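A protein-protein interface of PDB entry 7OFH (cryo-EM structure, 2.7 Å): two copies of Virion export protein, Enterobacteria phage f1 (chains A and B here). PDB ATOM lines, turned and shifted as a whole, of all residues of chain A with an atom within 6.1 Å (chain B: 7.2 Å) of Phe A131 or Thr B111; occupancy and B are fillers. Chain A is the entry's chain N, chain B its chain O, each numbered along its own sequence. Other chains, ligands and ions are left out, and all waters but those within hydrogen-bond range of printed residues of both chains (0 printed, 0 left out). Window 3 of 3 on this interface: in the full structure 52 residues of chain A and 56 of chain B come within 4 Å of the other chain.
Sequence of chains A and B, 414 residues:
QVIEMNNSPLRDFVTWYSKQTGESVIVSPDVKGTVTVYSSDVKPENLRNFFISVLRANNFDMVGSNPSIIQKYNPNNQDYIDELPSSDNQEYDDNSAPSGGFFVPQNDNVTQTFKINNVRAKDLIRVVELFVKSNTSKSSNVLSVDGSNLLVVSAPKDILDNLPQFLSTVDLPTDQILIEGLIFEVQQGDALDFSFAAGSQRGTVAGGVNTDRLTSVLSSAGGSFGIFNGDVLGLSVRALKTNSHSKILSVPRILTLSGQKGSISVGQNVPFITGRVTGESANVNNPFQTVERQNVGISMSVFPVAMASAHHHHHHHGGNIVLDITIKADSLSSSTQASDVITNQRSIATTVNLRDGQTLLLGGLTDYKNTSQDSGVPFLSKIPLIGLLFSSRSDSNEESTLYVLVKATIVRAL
The backbone carbonyl oxygen (O) of Asn B141 is in hydrogen-bond range of the backbone NH (N) of Ser B154 (2.9 Å). The side-chain hydroxyl (OG) of Ser B154 lies within hydrogen-bond range of the side-chain hydroxyl (OG1) of Thr B111, at 3.0 Å.
Val A127 touches Val B152. O of Leu A130 touches OG1 of Thr B111, at 3.96 Å. O of Asn B141 touches CD1 of Leu A130 (3.7 Å). Phe A131 touches Thr B111 (CD1 to CB, 3.6 Å). Phe A166 touches Thr B111 (CZ to CG2, 3.8 Å). Phe A166 touches Thr B113 (CE1 to CG2, 3.2 Å). Phe A166 touches Val B152 (CZ to CG1, 3.5 Å).
Of the printed residues of chain B, Leu A130 touches Thr B111 and Asn B141. Printed residues of chain B within 4 Å of Phe A131: Thr B111. Of chain A, only Leu A130 (3.96 Å), Phe A131 (3.6 Å) and Phe A166 (3.8 Å) come within 4 Å of Thr B111. Of the printed residues of chain A, Thr B113 touches Phe A166 (3.2 Å). Printed residues of chain A within 4 Å of Asn B141: Leu A130. Printed residues of chain A within 4 Å of Val B152: Val A127 (3.4 Å) and Phe A166 (3.5 Å). The nearest printed residue of chain B that does not touch Phe A131 is Ser B154 (6.0 Å).
Of the 12 printed residues of chain B, 4 touch a printed residue of chain A. Hydrophobic or aromatic side chains of chain A that line the printed part of chain B: Val A127, Leu A130, Phe A131 and Phe A166. Along chain A the printed residues that touch a printed residue of chain B span positions 127 to 166.
Position printed for both chains: 160.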
ATOM      1  N   ARG A 126       6.418  37.616  17.498  1.00  0.00           N
ATOM      2  CA  ARG A 126       6.386  37.179  16.118  1.00  0.00           C
ATOM      3  C   ARG A 126       6.592  35.678  16.048  1.00  0.00           C
ATOM      4  O   ARG A 126       5.965  34.988  15.240  1.00  0.00           O
ATOM      5  CB  ARG A 126       7.419  37.949  15.303  1.00  0.00           C
ATOM      6  CG  ARG A 126       7.001  39.376  14.996  1.00  0.00           C
ATOM      7  CD  ARG A 126       7.446  39.758  13.604  1.00  0.00           C
ATOM      8  NE  ARG A 126       6.813  41.010  13.182  1.00  0.00           N
ATOM      9  CZ  ARG A 126       6.576  41.383  11.920  1.00  0.00           C
ATOM     10  NH1 ARG A 126       6.917  40.596  10.910  1.00  0.00           N
ATOM     11  NH2 ARG A 126       5.996  42.548  11.672  1.00  0.00           N
ATOM     12  N   VAL A 127       7.493  35.188  16.880  1.00  0.00           N
ATOM     13  CA  VAL A 127       7.826  33.781  16.947  1.00  0.00           C
ATOM     14  C   VAL A 127       6.608  33.020  17.436  1.00  0.00           C
ATOM     15  O   VAL A 127       6.392  31.889  17.034  1.00  0.00           O
ATOM     16  CB  VAL A 127       8.975  33.552  17.934  1.00  0.00           C
ATOM     17  CG1 VAL A 127       9.490  32.147  17.840  1.00  0.00           C
ATOM     18  CG2 VAL A 127      10.122  34.501  17.694  1.00  0.00           C
ATOM     19  N   VAL A 128       5.862  33.609  18.365  1.00  0.00           N
ATOM     20  CA  VAL A 128       4.784  32.880  19.004  1.00  0.00           C
ATOM     21  C   VAL A 128       3.541  33.105  18.165  1.00  0.00           C
ATOM     22  O   VAL A 128       2.607  32.309  18.204  1.00  0.00           O
ATOM     23  CB  VAL A 128       4.630  33.248  20.492  1.00  0.00           C
ATOM     24  CG1 VAL A 128       3.478  32.539  21.154  1.00  0.00           C
ATOM     25  CG2 VAL A 128       5.879  32.899  21.279  1.00  0.00           C
ATOM     26  N   GLU A 129       3.588  34.138  17.326  1.00  0.00           N
ATOM     27  CA  GLU A 129       2.510  34.359  16.393  1.00  0.00           C
ATOM     28  C   GLU A 129       2.514  33.240  15.356  1.00  0.00           C
ATOM     29  O   GLU A 129       1.443  32.860  14.890  1.00  0.00           O
ATOM     30  CB  GLU A 129       2.583  35.767  15.810  1.00  0.00           C
ATOM     31  CG  GLU A 129       1.210  36.345  15.503  1.00  0.00           C
ATOM     32  CD  GLU A 129       0.565  37.162  16.620  1.00  0.00           C
ATOM     33  OE1 GLU A 129       1.304  37.950  17.252  1.00  0.00           O
ATOM     34  OE2 GLU A 129      -0.682  37.031  16.849  1.00  0.00           O
ATOM     35  N   LEU A 130       3.698  32.722  14.984  1.00  0.00           N
ATOM     36  CA  LEU A 130       3.826  31.602  14.063  1.00  0.00           C
ATOM     37  C   LEU A 130       3.336  30.320  14.711  1.00  0.00           C
ATOM     38  O   LEU A 130       2.694  29.517  14.038  1.00  0.00           O
ATOM     39  CB  LEU A 130       5.288  31.355  13.703  1.00  0.00           C
ATOM     40  CG  LEU A 130       5.898  32.079  12.505  1.00  0.00           C
ATOM     41  CD1 LEU A 130       7.183  31.358  12.107  1.00  0.00           C
ATOM     42  CD2 LEU A 130       4.968  32.081  11.297  1.00  0.00           C
ATOM     43  N   PHE A 131       3.732  30.065  15.955  1.00  0.00           N
ATOM     44  CA  PHE A 131       3.376  28.792  16.545  1.00  0.00           C
ATOM     45  C   PHE A 131       1.858  28.667  16.589  1.00  0.00           C
ATOM     46  O   PHE A 131       1.312  27.564  16.538  1.00  0.00           O
ATOM     47  CB  PHE A 131       3.952  28.660  17.950  1.00  0.00           C
ATOM     48  CG  PHE A 131       3.929  27.266  18.506  1.00  0.00           C
ATOM     49  CD1 PHE A 131       4.901  26.363  18.152  1.00  0.00           C
ATOM     50  CD2 PHE A 131       2.948  26.861  19.381  1.00  0.00           C
ATOM     51  CE1 PHE A 131       4.900  25.075  18.656  1.00  0.00           C
ATOM     52  CE2 PHE A 131       2.952  25.583  19.912  1.00  0.00           C
ATOM     53  CZ  PHE A 131       3.930  24.692  19.544  1.00  0.00           C
ATOM     54  N   VAL A 132       1.172  29.803  16.718  1.00  0.00           N
ATOM     55  CA  VAL A 132      -0.249  29.732  16.957  1.00  0.00           C
ATOM     56  C   VAL A 132      -0.979  29.937  15.645  1.00  0.00           C
ATOM     57  O   VAL A 132      -2.136  29.547  15.549  1.00  0.00           O
ATOM     58  CB  VAL A 132      -0.726  30.692  18.057  1.00  0.00           C
ATOM     59  CG1 VAL A 132       0.017  30.456  19.362  1.00  0.00           C
ATOM     60  CG2 VAL A 132      -0.628  32.150  17.628  1.00  0.00           C
ATOM     61  N   LYS A 133      -0.318  30.529  14.646  1.00  0.00           N
ATOM     62  CA  LYS A 133      -0.952  30.764  13.356  1.00  0.00           C
ATOM     63  C   LYS A 133      -1.499  29.449  12.798  1.00  0.00           C
ATOM     64  O   LYS A 133      -0.930  28.388  13.046  1.00  0.00           O
ATOM     65  CB  LYS A 133       0.040  31.390  12.371  1.00  0.00           C
ATOM     66  CG  LYS A 133      -0.512  31.694  10.985  1.00  0.00           C
ATOM     67  CD  LYS A 133       0.556  31.988   9.950  1.00  0.00           C
ATOM     68  CE  LYS A 133      -0.005  32.128   8.549  1.00  0.00           C
ATOM     69  NZ  LYS A 133       1.023  32.589   7.584  1.00  0.00           N
ATOM     70  N   ILE A 159      -2.960  23.506  20.610  1.00  0.00           N
ATOM     71  CA  ILE A 159      -1.838  24.368  20.300  1.00  0.00           C
ATOM     72  C   ILE A 159      -1.279  24.902  21.607  1.00  0.00           C
ATOM     73  O   ILE A 159      -0.065  24.932  21.785  1.00  0.00           O
ATOM     74  CB  ILE A 159      -2.208  25.486  19.306  1.00  0.00           C
ATOM     75  CG1 ILE A 159      -2.851  24.920  18.041  1.00  0.00           C
ATOM     76  CG2 ILE A 159      -0.986  26.319  18.938  1.00  0.00           C
ATOM     77  CD1 ILE A 159      -3.266  25.976  17.031  1.00  0.00           C
ATOM     78  N   LEU A 160      -2.159  25.284  22.526  1.00  0.00           N
ATOM     79  CA  LEU A 160      -1.715  25.948  23.739  1.00  0.00           C
ATOM     80  C   LEU A 160      -1.194  24.941  24.738  1.00  0.00           C
ATOM     81  O   LEU A 160      -0.834  25.320  25.850  1.00  0.00           O
ATOM     82  CB  LEU A 160      -2.846  26.797  24.329  1.00  0.00           C
ATOM     83  CG  LEU A 160      -3.168  28.052  23.517  1.00  0.00           C
ATOM     84  CD1 LEU A 160      -4.302  28.838  24.144  1.00  0.00           C
ATOM     85  CD2 LEU A 160      -1.938  28.931  23.346  1.00  0.00           C
ATOM     86  N   ASN A 162       1.215  22.721  23.694  1.00  0.00           N
ATOM     87  CA  ASN A 162       2.569  22.558  23.212  1.00  0.00           C
ATOM     88  C   ASN A 162       3.360  23.859  23.327  1.00  0.00           C
ATOM     89  O   ASN A 162       4.587  23.843  23.189  1.00  0.00           O
ATOM     90  CB  ASN A 162       2.559  22.057  21.769  1.00  0.00           C
ATOM     91  CG  ASN A 162       2.041  20.644  21.632  1.00  0.00           C
ATOM     92  OD1 ASN A 162       2.008  19.880  22.599  1.00  0.00           O
ATOM     93  ND2 ASN A 162       1.637  20.291  20.424  1.00  0.00           N
ATOM     94  N   LEU A 163       2.680  24.984  23.568  1.00  0.00           N
ATOM     95  CA  LEU A 163       3.382  26.250  23.683  1.00  0.00           C
ATOM     96  C   LEU A 163       4.389  26.214  24.818  1.00  0.00           C
ATOM     97  O   LEU A 163       5.478  26.735  24.655  1.00  0.00           O
ATOM     98  CB  LEU A 163       2.415  27.431  23.792  1.00  0.00           C
ATOM     99  CG  LEU A 163       3.029  28.819  23.636  1.00  0.00           C
ATOM    100  CD1 LEU A 163       1.977  29.776  23.107  1.00  0.00           C
ATOM    101  CD2 LEU A 163       3.467  29.317  24.995  1.00  0.00           C
ATOM    102  N   PHE A 166       7.711  25.087  23.371  1.00  0.00           N
ATOM    103  CA  PHE A 166       8.318  25.936  22.370  1.00  0.00           C
ATOM    104  C   PHE A 166       8.994  27.105  23.068  1.00  0.00           C
ATOM    105  O   PHE A 166       9.946  27.692  22.553  1.00  0.00           O
ATOM    106  CB  PHE A 166       7.269  26.543  21.448  1.00  0.00           C
ATOM    107  CG  PHE A 166       7.819  27.377  20.321  1.00  0.00           C
ATOM    108  CD1 PHE A 166       8.804  26.873  19.508  1.00  0.00           C
ATOM    109  CD2 PHE A 166       7.313  28.630  20.037  1.00  0.00           C
ATOM    110  CE1 PHE A 166       9.280  27.612  18.443  1.00  0.00           C
ATOM    111  CE2 PHE A 166       7.828  29.397  19.013  1.00  0.00           C
ATOM    112  CZ  PHE A 166       8.809  28.878  18.215  1.00  0.00           C
ATOM    113  N   ASN B 109       1.152  22.210  10.025  1.00  0.00           N
ATOM    114  CA  ASN B 109       2.518  22.676  10.079  1.00  0.00           C
ATOM    115  C   ASN B 109       3.009  22.585  11.512  1.00  0.00           C
ATOM    116  O   ASN B 109       2.390  23.135  12.422  1.00  0.00           O
ATOM    117  CB  ASN B 109       2.582  24.143   9.689  1.00  0.00           C
ATOM    118  CG  ASN B 109       2.298  24.388   8.228  1.00  0.00           C
ATOM    119  OD1 ASN B 109       2.294  23.465   7.432  1.00  0.00           O
ATOM    120  ND2 ASN B 109       2.096  25.638   7.853  1.00  0.00           N
ATOM    121  N   VAL B 110       4.141  21.919  11.710  1.00  0.00           N
ATOM    122  CA  VAL B 110       4.832  21.994  12.984  1.00  0.00           C
ATOM    123  C   VAL B 110       5.726  23.236  12.983  1.00  0.00           C
ATOM    124  O   VAL B 110       6.099  23.736  11.928  1.00  0.00           O
ATOM    125  CB  VAL B 110       5.641  20.711  13.205  1.00  0.00           C
ATOM    126  CG1 VAL B 110       6.111  20.575  14.645  1.00  0.00           C
ATOM    127  CG2 VAL B 110       4.834  19.491  12.808  1.00  0.00           C
ATOM    128  N   THR B 111       6.086  23.734  14.169  1.00  0.00           N
ATOM    129  CA  THR B 111       7.024  24.839  14.288  1.00  0.00           C
ATOM    130  C   THR B 111       8.196  24.400  15.158  1.00  0.00           C
ATOM    131  O   THR B 111       8.016  24.172  16.352  1.00  0.00           O
ATOM    132  CB  THR B 111       6.322  26.081  14.856  1.00  0.00           C
ATOM    133  OG1 THR B 111       5.305  26.537  13.962  1.00  0.00           O
ATOM    134  CG2 THR B 111       7.257  27.242  15.097  1.00  0.00           C
ATOM    135  N   GLN B 112       9.394  24.310  14.571  1.00  0.00           N
ATOM    136  CA  GLN B 112      10.581  23.986  15.344  1.00  0.00           C
ATOM    137  C   GLN B 112      11.564  25.157  15.351  1.00  0.00           C
ATOM    138  O   GLN B 112      11.466  26.069  14.538  1.00  0.00           O
ATOM    139  CB  GLN B 112      11.297  22.770  14.771  1.00  0.00           C
ATOM    140  CG  GLN B 112      10.640  21.444  15.094  1.00  0.00           C
ATOM    141  CD  GLN B 112      11.493  20.313  14.569  1.00  0.00           C
ATOM    142  OE1 GLN B 112      12.722  20.372  14.602  1.00  0.00           O
ATOM    143  NE2 GLN B 112      10.846  19.267  14.077  1.00  0.00           N
ATOM    144  N   THR B 113      12.534  25.095  16.271  1.00  0.00           N
ATOM    145  CA  THR B 113      13.653  26.010  16.299  1.00  0.00           C
ATOM    146  C   THR B 113      14.941  25.246  16.015  1.00  0.00           C
ATOM    147  O   THR B 113      15.144  24.148  16.538  1.00  0.00           O
ATOM    148  CB  THR B 113      13.747  26.740  17.641  1.00  0.00           C
ATOM    149  OG1 THR B 113      14.127  25.849  18.691  1.00  0.00           O
ATOM    150  CG2 THR B 113      12.433  27.371  18.037  1.00  0.00           C
ATOM    151  N   PHE B 114      15.813  25.876  15.216  1.00  0.00           N
ATOM    152  CA  PHE B 114      17.074  25.314  14.794  1.00  0.00           C
ATOM    153  C   PHE B 114      18.172  26.272  15.232  1.00  0.00           C
ATOM    154  O   PHE B 114      18.062  27.465  14.994  1.00  0.00           O
ATOM    155  CB  PHE B 114      17.045  25.173  13.275  1.00  0.00           C
ATOM    156  CG  PHE B 114      16.018  24.206  12.742  1.00  0.00           C
ATOM    157  CD1 PHE B 114      14.739  24.632  12.423  1.00  0.00           C
ATOM    158  CD2 PHE B 114      16.315  22.862  12.613  1.00  0.00           C
ATOM    159  CE1 PHE B 114      13.786  23.735  11.961  1.00  0.00           C
ATOM    160  CE2 PHE B 114      15.368  21.969  12.146  1.00  0.00           C
ATOM    161  CZ  PHE B 114      14.109  22.407  11.808  1.00  0.00           C
ATOM    162  N   ASN B 141       7.232  32.316   7.120  1.00  0.00           N
ATOM    163  CA  ASN B 141       7.165  30.975   7.649  1.00  0.00           C
ATOM    164  C   ASN B 141       8.494  30.701   8.326  1.00  0.00           C
ATOM    165  O   ASN B 141       8.617  29.763   9.102  1.00  0.00           O
ATOM    166  CB  ASN B 141       6.981  29.973   6.520  1.00  0.00           C
ATOM    167  CG  ASN B 141       5.605  29.352   6.479  1.00  0.00           C
ATOM    168  OD1 ASN B 141       4.721  29.726   7.251  1.00  0.00           O
ATOM    169  ND2 ASN B 141       5.427  28.378   5.600  1.00  0.00           N
ATOM    170  N   VAL B 152      13.254  29.926  13.641  1.00  0.00           N
ATOM    171  CA  VAL B 152      11.970  29.305  13.880  1.00  0.00           C
ATOM    172  C   VAL B 152      11.299  29.118  12.523  1.00  0.00           C
ATOM    173  O   VAL B 152      10.988  30.105  11.882  1.00  0.00           O
ATOM    174  CB  VAL B 152      11.144  30.160  14.852  1.00  0.00           C
ATOM    175  CG1 VAL B 152       9.703  29.695  14.952  1.00  0.00           C
ATOM    176  CG2 VAL B 152      11.746  30.151  16.242  1.00  0.00           C
ATOM    177  N   VAL B 153      11.073  27.862  12.087  1.00  0.00           N
ATOM    178  CA  VAL B 153      10.470  27.554  10.794  1.00  0.00           C
ATOM    179  C   VAL B 153       9.142  26.817  10.994  1.00  0.00           C
ATOM    180  O   VAL B 153       9.036  25.936  11.832  1.00  0.00           O
ATOM    181  CB  VAL B 153      11.425  26.776   9.874  1.00  0.00           C
ATOM    182  CG1 VAL B 153      12.868  27.247   9.998  1.00  0.00           C
ATOM    183  CG2 VAL B 153      11.397  25.299  10.148  1.00  0.00           C
ATOM    184  N   SER B 154       8.108  27.174  10.221  1.00  0.00           N
ATOM    185  CA  SER B 154       6.839  26.465  10.246  1.00  0.00           C
ATOM    186  C   SER B 154       6.585  25.833   8.885  1.00  0.00           C
ATOM    187  O   SER B 154       6.432  26.565   7.911  1.00  0.00           O
ATOM    188  CB  SER B 154       5.729  27.402  10.548  1.00  0.00           C
ATOM    189  OG  SER B 154       4.600  26.692  11.052  1.00  0.00           O
ATOM    190  N   ALA B 155       6.535  24.490   8.821  1.00  0.00           N
ATOM    191  CA  ALA B 155       6.377  23.772   7.571  1.00  0.00           C
ATOM    192  C   ALA B 155       5.923  22.361   7.893  1.00  0.00           C
ATOM    193  O   ALA B 155       6.009  21.969   9.039  1.00  0.00           O
ATOM    194  CB  ALA B 155       7.710  23.753   6.862  1.00  0.00           C
ATOM    195  N   LEU B 160      10.290  19.418   7.503  1.00  0.00           N
ATOM    196  CA  LEU B 160      11.069  19.823   8.659  1.00  0.00           C
ATOM    197  C   LEU B 160      11.932  18.685   9.150  1.00  0.00           C
ATOM    198  O   LEU B 160      12.614  18.836  10.160  1.00  0.00           O
ATOM    199  CB  LEU B 160      10.154  20.356   9.767  1.00  0.00           C
ATOM    200  CG  LEU B 160       9.537  21.718   9.449  1.00  0.00           C
ATOM    201  CD1 LEU B 160       8.628  22.188  10.563  1.00  0.00           C
ATOM    202  CD2 LEU B 160      10.607  22.760   9.161  1.00  0.00           C
